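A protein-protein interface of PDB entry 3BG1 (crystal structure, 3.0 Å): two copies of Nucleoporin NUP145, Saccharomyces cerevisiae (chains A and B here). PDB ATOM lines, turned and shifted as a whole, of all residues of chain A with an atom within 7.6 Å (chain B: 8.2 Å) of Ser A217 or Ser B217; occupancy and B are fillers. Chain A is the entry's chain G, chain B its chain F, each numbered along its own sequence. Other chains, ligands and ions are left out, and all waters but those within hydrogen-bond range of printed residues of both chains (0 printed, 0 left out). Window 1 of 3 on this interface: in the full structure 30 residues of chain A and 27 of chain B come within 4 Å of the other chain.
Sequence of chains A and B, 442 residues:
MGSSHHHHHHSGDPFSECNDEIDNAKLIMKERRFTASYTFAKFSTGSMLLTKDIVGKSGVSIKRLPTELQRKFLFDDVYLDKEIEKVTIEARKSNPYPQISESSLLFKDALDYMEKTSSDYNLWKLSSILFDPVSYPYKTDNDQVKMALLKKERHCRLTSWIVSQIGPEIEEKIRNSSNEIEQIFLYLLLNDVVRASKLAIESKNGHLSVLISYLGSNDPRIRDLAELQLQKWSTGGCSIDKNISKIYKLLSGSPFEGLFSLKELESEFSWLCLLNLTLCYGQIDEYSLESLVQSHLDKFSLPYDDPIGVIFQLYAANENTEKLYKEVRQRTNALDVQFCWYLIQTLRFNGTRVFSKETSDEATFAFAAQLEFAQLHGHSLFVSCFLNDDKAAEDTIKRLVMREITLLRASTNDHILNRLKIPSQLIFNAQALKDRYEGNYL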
ATOM      1  N   LYS A 152      14.501 -10.167   0.077  1.00  0.00           N
ATOM      2  CA  LYS A 152      14.436 -10.620   1.461  1.00  0.00           C
ATOM      3  C   LYS A 152      15.804 -10.703   2.147  1.00  0.00           C
ATOM      4  O   LYS A 152      15.949 -10.228   3.273  1.00  0.00           O
ATOM      5  CB  LYS A 152      13.734 -11.984   1.543  1.00  0.00           C
ATOM      6  CG  LYS A 152      13.425 -12.443   2.966  1.00  0.00           C
ATOM      7  CD  LYS A 152      11.941 -12.725   3.166  1.00  0.00           C
ATOM      8  CE  LYS A 152      11.522 -12.489   4.621  1.00  0.00           C
ATOM      9  NZ  LYS A 152      10.056 -12.679   4.864  1.00  0.00           N
ATOM     10  N   LEU A 211      -1.380 -17.167  17.582  1.00  0.00           N
ATOM     11  CA  LEU A 211      -1.274 -15.950  16.785  1.00  0.00           C
ATOM     12  C   LEU A 211       0.192 -15.728  16.476  1.00  0.00           C
ATOM     13  O   LEU A 211       0.567 -15.584  15.313  1.00  0.00           O
ATOM     14  CB  LEU A 211      -1.840 -14.762  17.556  1.00  0.00           C
ATOM     15  CG  LEU A 211      -3.000 -15.150  18.484  1.00  0.00           C
ATOM     16  CD1 LEU A 211      -3.686 -13.904  19.010  1.00  0.00           C
ATOM     17  CD2 LEU A 211      -3.995 -16.022  17.739  1.00  0.00           C
ATOM     18  N   ILE A 212       1.016 -15.715  17.523  1.00  0.00           N
ATOM     19  CA  ILE A 212       2.457 -15.547  17.379  1.00  0.00           C
ATOM     20  C   ILE A 212       2.952 -16.423  16.235  1.00  0.00           C
ATOM     21  O   ILE A 212       3.883 -16.061  15.523  1.00  0.00           O
ATOM     22  CB  ILE A 212       3.188 -15.959  18.670  1.00  0.00           C
ATOM     23  CG1 ILE A 212       3.091 -14.830  19.685  1.00  0.00           C
ATOM     24  CG2 ILE A 212       4.633 -16.305  18.378  1.00  0.00           C
ATOM     25  CD1 ILE A 212       3.827 -15.109  20.962  1.00  0.00           C
ATOM     26  N   SER A 213       2.322 -17.583  16.075  1.00  0.00           N
ATOM     27  CA  SER A 213       2.679 -18.505  15.011  1.00  0.00           C
ATOM     28  C   SER A 213       2.434 -17.847  13.671  1.00  0.00           C
ATOM     29  O   SER A 213       3.277 -17.891  12.776  1.00  0.00           O
ATOM     30  CB  SER A 213       1.827 -19.762  15.084  1.00  0.00           C
ATOM     31  OG  SER A 213       1.906 -20.476  13.862  1.00  0.00           O
ATOM     32  N   TYR A 214       1.256 -17.248  13.545  1.00  0.00           N
ATOM     33  CA  TYR A 214       0.839 -16.574  12.321  1.00  0.00           C
ATOM     34  C   TYR A 214       1.587 -15.271  12.066  1.00  0.00           C
ATOM     35  O   TYR A 214       1.871 -14.903  10.919  1.00  0.00           O
ATOM     36  CB  TYR A 214      -0.672 -16.317  12.384  1.00  0.00           C
ATOM     37  CG  TYR A 214      -1.470 -17.575  12.150  1.00  0.00           C
ATOM     38  CD1 TYR A 214      -2.616 -17.860  12.896  1.00  0.00           C
ATOM     39  CD2 TYR A 214      -1.052 -18.500  11.194  1.00  0.00           C
ATOM     40  CE1 TYR A 214      -3.319 -19.043  12.692  1.00  0.00           C
ATOM     41  CE2 TYR A 214      -1.741 -19.676  10.982  1.00  0.00           C
ATOM     42  CZ  TYR A 214      -2.868 -19.945  11.730  1.00  0.00           C
ATOM     43  OH  TYR A 214      -3.520 -21.132  11.507  1.00  0.00           O
ATOM     44  N   LEU A 215       1.910 -14.586  13.155  1.00  0.00           N
ATOM     45  CA  LEU A 215       2.608 -13.308  13.111  1.00  0.00           C
ATOM     46  C   LEU A 215       3.652 -13.214  12.006  1.00  0.00           C
ATOM     47  O   LEU A 215       3.644 -12.264  11.227  1.00  0.00           O
ATOM     48  CB  LEU A 215       3.251 -13.041  14.475  1.00  0.00           C
ATOM     49  CG  LEU A 215       3.858 -11.668  14.762  1.00  0.00           C
ATOM     50  CD1 LEU A 215       2.817 -10.562  14.584  1.00  0.00           C
ATOM     51  CD2 LEU A 215       4.403 -11.679  16.184  1.00  0.00           C
ATOM     52  N   GLY A 216       4.532 -14.205  11.927  1.00  0.00           N
ATOM     53  CA  GLY A 216       5.572 -14.186  10.913  1.00  0.00           C
ATOM     54  C   GLY A 216       5.098 -14.154   9.469  1.00  0.00           C
ATOM     55  O   GLY A 216       5.823 -13.690   8.584  1.00  0.00           O
ATOM     56  N   SER A 217       3.887 -14.636   9.218  1.00  0.00           N
ATOM     57  CA  SER A 217       3.363 -14.667   7.859  1.00  0.00           C
ATOM     58  C   SER A 217       2.470 -13.482   7.551  1.00  0.00           C
ATOM     59  O   SER A 217       2.462 -12.478   8.265  1.00  0.00           O
ATOM     60  CB  SER A 217       2.572 -15.957   7.634  1.00  0.00           C
ATOM     61  OG  SER A 217       3.361 -17.097   7.925  1.00  0.00           O
ATOM     62  N   ASN A 218       1.718 -13.612   6.468  1.00  0.00           N
ATOM     63  CA  ASN A 218       0.799 -12.571   6.063  1.00  0.00           C
ATOM     64  C   ASN A 218      -0.513 -13.221   5.653  1.00  0.00           C
ATOM     65  O   ASN A 218      -0.728 -13.539   4.483  1.00  0.00           O
ATOM     66  CB  ASN A 218       1.378 -11.766   4.899  1.00  0.00           C
ATOM     67  CG  ASN A 218       0.751 -10.390   4.781  1.00  0.00           C
ATOM     68  OD1 ASN A 218      -0.462 -10.254   4.602  1.00  0.00           O
ATOM     69  ND2 ASN A 218       1.577  -9.357   4.892  1.00  0.00           N
ATOM     70  N   ASP A 219      -1.382 -13.442   6.631  1.00  0.00           N
ATOM     71  CA  ASP A 219      -2.678 -14.041   6.365  1.00  0.00           C
ATOM     72  C   ASP A 219      -3.783 -13.084   6.786  1.00  0.00           C
ATOM     73  O   ASP A 219      -3.946 -12.769   7.969  1.00  0.00           O
ATOM     74  CB  ASP A 219      -2.841 -15.365   7.113  1.00  0.00           C
ATOM     75  CG  ASP A 219      -4.114 -16.097   6.722  1.00  0.00           C
ATOM     76  OD1 ASP A 219      -5.191 -15.468   6.741  1.00  0.00           O
ATOM     77  OD2 ASP A 219      -4.043 -17.300   6.397  1.00  0.00           O
ATOM     78  N   PRO A 220      -4.561 -12.607   5.812  1.00  0.00           N
ATOM     79  CA  PRO A 220      -5.665 -11.680   6.053  1.00  0.00           C
ATOM     80  C   PRO A 220      -6.697 -12.205   7.054  1.00  0.00           C
ATOM     81  O   PRO A 220      -7.243 -11.433   7.843  1.00  0.00           O
ATOM     82  CB  PRO A 220      -6.242 -11.473   4.657  1.00  0.00           C
ATOM     83  CG  PRO A 220      -5.926 -12.778   3.966  1.00  0.00           C
ATOM     84  CD  PRO A 220      -4.513 -13.011   4.395  1.00  0.00           C
ATOM     85  N   ILE A 222      -6.416 -13.865   9.777  1.00  0.00           N
ATOM     86  CA  ILE A 222      -5.894 -13.427  11.057  1.00  0.00           C
ATOM     87  C   ILE A 222      -5.978 -11.918  11.161  1.00  0.00           C
ATOM     88  O   ILE A 222      -6.701 -11.378  11.998  1.00  0.00           O
ATOM     89  CB  ILE A 222      -4.426 -13.869  11.203  1.00  0.00           C
ATOM     90  CG1 ILE A 222      -4.355 -15.384  11.380  1.00  0.00           C
ATOM     91  CG2 ILE A 222      -3.774 -13.153  12.361  1.00  0.00           C
ATOM     92  CD1 ILE A 222      -4.759 -16.157  10.152  1.00  0.00           C
ATOM     93  N   ARG A 223      -5.224 -11.248  10.299  1.00  0.00           N
ATOM     94  CA  ARG A 223      -5.189  -9.799  10.260  1.00  0.00           C
ATOM     95  C   ARG A 223      -6.554  -9.243  10.664  1.00  0.00           C
ATOM     96  O   ARG A 223      -6.680  -8.548  11.675  1.00  0.00           O
ATOM     97  CB  ARG A 223      -4.815  -9.358   8.849  1.00  0.00           C
ATOM     98  CG  ARG A 223      -4.263  -7.964   8.739  1.00  0.00           C
ATOM     99  CD  ARG A 223      -3.569  -7.819   7.408  1.00  0.00           C
ATOM    100  NE  ARG A 223      -2.971  -6.503   7.237  1.00  0.00           N
ATOM    101  CZ  ARG A 223      -2.144  -6.192   6.246  1.00  0.00           C
ATOM    102  NH1 ARG A 223      -1.824  -7.113   5.344  1.00  0.00           N
ATOM    103  NH2 ARG A 223      -1.637  -4.965   6.156  1.00  0.00           N
ATOM    104  N   LEU A 250       0.211  -6.078  16.884  1.00  0.00           N
ATOM    105  CA  LEU A 250       1.297  -6.505  16.012  1.00  0.00           C
ATOM    106  C   LEU A 250       0.796  -7.375  14.871  1.00  0.00           C
ATOM    107  O   LEU A 250       1.542  -7.666  13.939  1.00  0.00           O
ATOM    108  CB  LEU A 250       2.361  -7.272  16.798  1.00  0.00           C
ATOM    109  CG  LEU A 250       3.037  -6.541  17.956  1.00  0.00           C
ATOM    110  CD1 LEU A 250       4.158  -7.411  18.491  1.00  0.00           C
ATOM    111  CD2 LEU A 250       3.581  -5.204  17.498  1.00  0.00           C
ATOM    112  N   LEU A 251      -0.461  -7.795  14.940  1.00  0.00           N
ATOM    113  CA  LEU A 251      -1.024  -8.623  13.884  1.00  0.00           C
ATOM    114  C   LEU A 251      -1.770  -7.774  12.878  1.00  0.00           C
ATOM    115  O   LEU A 251      -1.711  -8.024  11.674  1.00  0.00           O
ATOM    116  CB  LEU A 251      -1.972  -9.665  14.468  1.00  0.00           C
ATOM    117  CG  LEU A 251      -1.243 -10.735  15.275  1.00  0.00           C
ATOM    118  CD1 LEU A 251      -2.228 -11.711  15.874  1.00  0.00           C
ATOM    119  CD2 LEU A 251      -0.268 -11.458  14.368  1.00  0.00           C
ATOM    120  N   CYS A 280       9.229  -5.310  10.812  1.00  0.00           N
ATOM    121  CA  CYS A 280       8.883  -6.706  11.054  1.00  0.00           C
ATOM    122  C   CYS A 280       7.395  -6.987  10.988  1.00  0.00           C
ATOM    123  O   CYS A 280       6.969  -7.937  10.339  1.00  0.00           O
ATOM    124  CB  CYS A 280       9.401  -7.168  12.419  1.00  0.00           C
ATOM    125  SG  CYS A 280      11.151  -7.592  12.495  1.00  0.00           S
ATOM    126  N   TYR A 281       6.601  -6.173  11.672  1.00  0.00           N
ATOM    127  CA  TYR A 281       5.167  -6.384  11.690  1.00  0.00           C
ATOM    128  C   TYR A 281       4.457  -5.304  10.927  1.00  0.00           C
ATOM    129  O   TYR A 281       3.270  -5.412  10.654  1.00  0.00           O
ATOM    130  CB  TYR A 281       4.668  -6.396  13.130  1.00  0.00           C
ATOM    131  CG  TYR A 281       5.535  -7.239  14.008  1.00  0.00           C
ATOM    132  CD1 TYR A 281       6.189  -6.693  15.106  1.00  0.00           C
ATOM    133  CD2 TYR A 281       5.772  -8.571  13.693  1.00  0.00           C
ATOM    134  CE1 TYR A 281       7.071  -7.453  15.868  1.00  0.00           C
ATOM    135  CE2 TYR A 281       6.648  -9.345  14.439  1.00  0.00           C
ATOM    136  CZ  TYR A 281       7.301  -8.783  15.525  1.00  0.00           C
ATOM    137  OH  TYR A 281       8.205  -9.547  16.241  1.00  0.00           O
ATOM    138  N   LYS B 152      -4.560 -25.191  14.538  1.00  0.00           N
ATOM    139  CA  LYS B 152      -3.173 -24.822  14.818  1.00  0.00           C
ATOM    140  C   LYS B 152      -2.815 -24.845  16.309  1.00  0.00           C
ATOM    141  O   LYS B 152      -1.779 -25.398  16.681  1.00  0.00           O
ATOM    142  CB  LYS B 152      -2.862 -23.436  14.232  1.00  0.00           C
ATOM    143  CG  LYS B 152      -1.387 -23.057  14.284  1.00  0.00           C
ATOM    144  CD  LYS B 152      -0.837 -22.725  12.902  1.00  0.00           C
ATOM    145  CE  LYS B 152       0.662 -23.031  12.813  1.00  0.00           C
ATOM    146  NZ  LYS B 152       1.243 -22.790  11.450  1.00  0.00           N
ATOM    147  N   LEU B 211      16.269 -18.577   3.353  1.00  0.00           N
ATOM    148  CA  LEU B 211      15.416 -19.750   3.211  1.00  0.00           C
ATOM    149  C   LEU B 211      14.763 -20.005   4.551  1.00  0.00           C
ATOM    150  O   LEU B 211      13.541 -20.094   4.637  1.00  0.00           O
ATOM    151  CB  LEU B 211      16.240 -20.959   2.787  1.00  0.00           C
ATOM    152  CG  LEU B 211      17.431 -20.582   1.893  1.00  0.00           C
ATOM    153  CD1 LEU B 211      18.047 -21.831   1.290  1.00  0.00           C
ATOM    154  CD2 LEU B 211      16.984 -19.633   0.792  1.00  0.00           C
ATOM    155  N   ILE B 212      15.584 -20.107   5.594  1.00  0.00           N
ATOM    156  CA  ILE B 212      15.097 -20.317   6.952  1.00  0.00           C
ATOM    157  C   ILE B 212      13.907 -19.395   7.208  1.00  0.00           C
ATOM    158  O   ILE B 212      12.976 -19.749   7.929  1.00  0.00           O
ATOM    159  CB  ILE B 212      16.198 -20.007   7.982  1.00  0.00           C
ATOM    160  CG1 ILE B 212      17.150 -21.187   8.075  1.00  0.00           C
ATOM    161  CG2 ILE B 212      15.590 -19.696   9.335  1.00  0.00           C
ATOM    162  CD1 ILE B 212      18.232 -21.008   9.101  1.00  0.00           C
ATOM    163  N   SER B 213      13.954 -18.206   6.615  1.00  0.00           N
ATOM    164  CA  SER B 213      12.881 -17.240   6.757  1.00  0.00           C
ATOM    165  C   SER B 213      11.609 -17.811   6.176  1.00  0.00           C
ATOM    166  O   SER B 213      10.545 -17.746   6.789  1.00  0.00           O
ATOM    167  CB  SER B 213      13.214 -15.960   6.003  1.00  0.00           C
ATOM    168  OG  SER B 213      12.045 -15.181   5.830  1.00  0.00           O
ATOM    169  N   TYR B 214      11.735 -18.357   4.973  1.00  0.00           N
ATOM    170  CA  TYR B 214      10.615 -18.947   4.251  1.00  0.00           C
ATOM    171  C   TYR B 214      10.131 -20.261   4.857  1.00  0.00           C
ATOM    172  O   TYR B 214       8.933 -20.571   4.850  1.00  0.00           O
ATOM    173  CB  TYR B 214      11.021 -19.153   2.787  1.00  0.00           C
ATOM    174  CG  TYR B 214      11.041 -17.857   2.019  1.00  0.00           C
ATOM    175  CD1 TYR B 214      12.049 -17.574   1.092  1.00  0.00           C
ATOM    176  CD2 TYR B 214      10.055 -16.894   2.247  1.00  0.00           C
ATOM    177  CE1 TYR B 214      12.072 -16.357   0.417  1.00  0.00           C
ATOM    178  CE2 TYR B 214      10.067 -15.685   1.585  1.00  0.00           C
ATOM    179  CZ  TYR B 214      11.073 -15.419   0.676  1.00  0.00           C
ATOM    180  OH  TYR B 214      11.066 -14.199   0.047  1.00  0.00           O
ATOM    181  N   LEU B 215      11.079 -21.017   5.392  1.00  0.00           N
ATOM    182  CA  LEU B 215      10.814 -22.314   5.997  1.00  0.00           C
ATOM    183  C   LEU B 215       9.489 -22.383   6.749  1.00  0.00           C
ATOM    184  O   LEU B 215       8.688 -23.286   6.516  1.00  0.00           O
ATOM    185  CB  LEU B 215      11.974 -22.680   6.927  1.00  0.00           C
ATOM    186  CG  LEU B 215      12.043 -24.088   7.515  1.00  0.00           C
ATOM    187  CD1 LEU B 215      12.064 -25.145   6.409  1.00  0.00           C
ATOM    188  CD2 LEU B 215      13.296 -24.177   8.378  1.00  0.00           C
ATOM    189  N   GLY B 216       9.250 -21.421   7.631  1.00  0.00           N
ATOM    190  CA  GLY B 216       8.020 -21.421   8.404  1.00  0.00           C
ATOM    191  C   GLY B 216       6.728 -21.355   7.606  1.00  0.00           C
ATOM    192  O   GLY B 216       5.677 -21.791   8.080  1.00  0.00           O
ATOM    193  N   SER B 217       6.792 -20.816   6.395  1.00  0.00           N
ATOM    194  CA  SER B 217       5.597 -20.688   5.572  1.00  0.00           C
ATOM    195  C   SER B 217       5.453 -21.821   4.577  1.00  0.00           C
ATOM    196  O   SER B 217       6.101 -22.863   4.690  1.00  0.00           O
ATOM    197  CB  SER B 217       5.625 -19.360   4.813  1.00  0.00           C
ATOM    198  OG  SER B 217       5.775 -18.268   5.701  1.00  0.00           O
ATOM    199  N   ASN B 218       4.584 -21.602   3.598  1.00  0.00           N
ATOM    200  CA  ASN B 218       4.359 -22.584   2.560  1.00  0.00           C
ATOM    201  C   ASN B 218       4.300 -21.864   1.220  1.00  0.00           C
ATOM    202  O   ASN B 218       3.232 -21.475   0.754  1.00  0.00           O
ATOM    203  CB  ASN B 218       3.055 -23.342   2.813  1.00  0.00           C
ATOM    204  CG  ASN B 218       3.025 -24.687   2.110  1.00  0.00           C
ATOM    205  OD1 ASN B 218       3.131 -24.769   0.883  1.00  0.00           O
ATOM    206  ND2 ASN B 218       2.889 -25.754   2.888  1.00  0.00           N
ATOM    207  N   ASP B 219       5.467 -21.670   0.615  1.00  0.00           N
ATOM    208  CA  ASP B 219       5.542 -21.011  -0.677  1.00  0.00           C
ATOM    209  C   ASP B 219       6.168 -21.952  -1.698  1.00  0.00           C
ATOM    210  O   ASP B 219       7.339 -22.325  -1.596  1.00  0.00           O
ATOM    211  CB  ASP B 219       6.368 -19.728  -0.597  1.00  0.00           C
ATOM    212  CG  ASP B 219       6.325 -18.930  -1.888  1.00  0.00           C
ATOM    213  OD1 ASP B 219       6.567 -19.521  -2.959  1.00  0.00           O
ATOM    214  OD2 ASP B 219       6.049 -17.715  -1.838  1.00  0.00           O
ATOM    215  N   PRO B 220       5.382 -22.345  -2.702  1.00  0.00           N
ATOM    216  CA  PRO B 220       5.833 -23.245  -3.763  1.00  0.00           C
ATOM    217  C   PRO B 220       7.071 -22.740  -4.504  1.00  0.00           C
ATOM    218  O   PRO B 220       7.930 -23.534  -4.887  1.00  0.00           O
ATOM    219  CB  PRO B 220       4.605 -23.350  -4.657  1.00  0.00           C
ATOM    220  CG  PRO B 220       3.922 -22.023  -4.451  1.00  0.00           C
ATOM    221  CD  PRO B 220       4.016 -21.864  -2.967  1.00  0.00           C
ATOM    222  N   ILE B 222       9.726 -21.250  -3.519  1.00  0.00           N
ATOM    223  CA  ILE B 222      10.825 -21.776  -2.734  1.00  0.00           C
ATOM    224  C   ILE B 222      10.877 -23.287  -2.863  1.00  0.00           C
ATOM    225  O   ILE B 222      11.835 -23.848  -3.397  1.00  0.00           O
ATOM    226  CB  ILE B 222      10.643 -21.396  -1.252  1.00  0.00           C
ATOM    227  CG1 ILE B 222      10.870 -19.896  -1.070  1.00  0.00           C
ATOM    228  CG2 ILE B 222      11.580 -22.197  -0.383  1.00  0.00           C
ATOM    229  CD1 ILE B 222       9.807 -19.041  -1.712  1.00  0.00           C
ATOM    230  N   ARG B 223       9.830 -23.932  -2.365  1.00  0.00           N
ATOM    231  CA  ARG B 223       9.716 -25.376  -2.407  1.00  0.00           C
ATOM    232  C   ARG B 223      10.405 -25.904  -3.667  1.00  0.00           C
ATOM    233  O   ARG B 223      11.385 -26.650  -3.587  1.00  0.00           O
ATOM    234  CB  ARG B 223       8.237 -25.749  -2.395  1.00  0.00           C
ATOM    235  CG  ARG B 223       7.935 -27.151  -1.951  1.00  0.00           C
ATOM    236  CD  ARG B 223       6.474 -27.244  -1.595  1.00  0.00           C
ATOM    237  NE  ARG B 223       6.106 -28.570  -1.117  1.00  0.00           N
ATOM    238  CZ  ARG B 223       4.934 -28.855  -0.559  1.00  0.00           C
ATOM    239  NH1 ARG B 223       4.025 -27.895  -0.415  1.00  0.00           N
ATOM    240  NH2 ARG B 223       4.669 -30.093  -0.148  1.00  0.00           N
ATOM    241  N   LEU B 250      14.694 -29.699   3.978  1.00  0.00           N
ATOM    242  CA  LEU B 250      13.639 -29.251   4.878  1.00  0.00           C
ATOM    243  C   LEU B 250      12.709 -28.255   4.205  1.00  0.00           C
ATOM    244  O   LEU B 250      11.660 -27.917   4.749  1.00  0.00           O
ATOM    245  CB  LEU B 250      14.222 -28.618   6.141  1.00  0.00           C
ATOM    246  CG  LEU B 250      15.140 -29.490   6.994  1.00  0.00           C
ATOM    247  CD1 LEU B 250      15.478 -28.734   8.266  1.00  0.00           C
ATOM    248  CD2 LEU B 250      14.469 -30.808   7.327  1.00  0.00           C
ATOM    249  N   LEU B 251      13.090 -27.777   3.028  1.00  0.00           N
ATOM    250  CA  LEU B 251      12.252 -26.827   2.310  1.00  0.00           C
ATOM    251  C   LEU B 251      11.377 -27.540   1.303  1.00  0.00           C
ATOM    252  O   LEU B 251      10.214 -27.184   1.118  1.00  0.00           O
ATOM    253  CB  LEU B 251      13.112 -25.795   1.590  1.00  0.00           C
ATOM    254  CG  LEU B 251      13.818 -24.846   2.552  1.00  0.00           C
ATOM    255  CD1 LEU B 251      14.696 -23.877   1.794  1.00  0.00           C
ATOM    256  CD2 LEU B 251      12.776 -24.095   3.355  1.00  0.00           C
ATOM    257  N   CYS B 280       6.662 -30.296  11.528  1.00  0.00           N
ATOM    258  CA  CYS B 280       7.046 -28.901  11.334  1.00  0.00           C
ATOM    259  C   CYS B 280       7.328 -28.537   9.890  1.00  0.00           C
ATOM    260  O   CYS B 280       6.838 -27.525   9.396  1.00  0.00           O
ATOM    261  CB  CYS B 280       8.283 -28.554  12.166  1.00  0.00           C
ATOM    262  SG  CYS B 280       7.991 -28.228  13.914  1.00  0.00           S
ATOM    263  N   TYR B 281       8.128 -29.352   9.215  1.00  0.00           N
ATOM    264  CA  TYR B 281       8.476 -29.068   7.834  1.00  0.00           C
ATOM    265  C   TYR B 281       7.833 -30.058   6.902  1.00  0.00           C
ATOM    266  O   TYR B 281       7.835 -29.870   5.693  1.00  0.00           O
ATOM    267  CB  TYR B 281       9.990 -29.125   7.665  1.00  0.00           C
ATOM    268  CG  TYR B 281      10.696 -28.388   8.755  1.00  0.00           C
ATOM    269  CD1 TYR B 281      11.590 -29.038   9.596  1.00  0.00           C
ATOM    270  CD2 TYR B 281      10.405 -27.051   9.005  1.00  0.00           C
ATOM    271  CE1 TYR B 281      12.175 -28.375  10.670  1.00  0.00           C
ATOM    272  CE2 TYR B 281      10.976 -26.373  10.072  1.00  0.00           C
ATOM    273  CZ  TYR B 281      11.860 -27.039  10.908  1.00  0.00           C
ATOM    274  OH  TYR B 281      12.398 -26.373  11.991  1.00  0.00           O
ATOM    275  N   GLN B 283       4.689 -30.777   6.241  1.00  0.00           N
ATOM    276  CA  GLN B 283       3.274 -30.540   5.955  1.00  0.00           C
ATOM    277  C   GLN B 283       2.950 -30.863   4.499  1.00  0.00           C
ATOM    278  O   GLN B 283       2.120 -30.192   3.863  1.00  0.00           O
ATOM    279  CB  GLN B 283       2.889 -29.090   6.302  1.00  0.00           C
ATOM    280  CG  GLN B 283       2.185 -28.915   7.659  1.00  0.00           C
ATOM    281  CD  GLN B 283       0.683 -28.651   7.523  1.00  0.00           C
ATOM    282  OE1 GLN B 283      -0.010 -29.333   6.768  1.00  0.00           O
ATOM    283  NE2 GLN B 283       0.176 -27.665   8.266  1.00  0.00           N
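Hydrophobic or aromatic side chains of chain B within 4 Å of the printed part of chain A: Tyr B214.
Along chain B the printed residues that touch a printed residue of chain A span positions 152 to 217.
Of the 17 printed residues of chain A, 4 touch a printed residue of chain B.
Printed residues of chain A that touch a printed residue of chain B: Lys A152, Ser A213, Tyr A214 and Ser A217.
Hydrophobic or aromatic side chains of chain A that line the printed part of chain B: Tyr A214.
Among the printed residues, no Asp or Glu carboxylate lies within 4 Å of a Lys or Arg side-chain nitrogen of the other chain.
Lys A152 touches Ser B213, and with the chains exchanged Ser A213 touches Lys B152.
Lys A152 touches Tyr B214, and with the chains exchanged Tyr A214 touches Lys B152.
Ser B217 touches its own counterpart, Ser A217.
Among the printed residues, merely in contact across the chains: Tyr A214 with Lys B152 and Lys A152 with Tyr B214.
The side-chain amino group (NZ) of Lys B152 lies close to the side-chain hydroxyl (OG) of Ser A213, 3.4 Å away.
OG of Ser B213 lies close to NZ of Lys A152.
OG of Ser A217 lies within hydrogen-bond range of OG of Ser B217, at 3.5 Å.
Of the printed residues of chain B, Lys A152 touches Ser B213 (3.0 Å) and Tyr B214 (3.6 Å).
Of the printed residues of chain B, Ser A213 touches Lys B152.
Of the printed residues of chain B, Tyr A214 touches Lys B152 (3.4 Å).
Ser A217 touches just one residue of chain B: Ser B217.
Tyr A281 touches none of the printed residues of chain B.
Of the printed residues of chain A, Ser B213 touches Lys A152.
Printed residues of chain A within 4 Å of Tyr B214: Lys A152 (3.6 Å).
Of chain A, only Ser A217 (3.5 Å) comes within 4 Å of Ser B217.
Leu B251 touches none of the printed residues of chain A.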
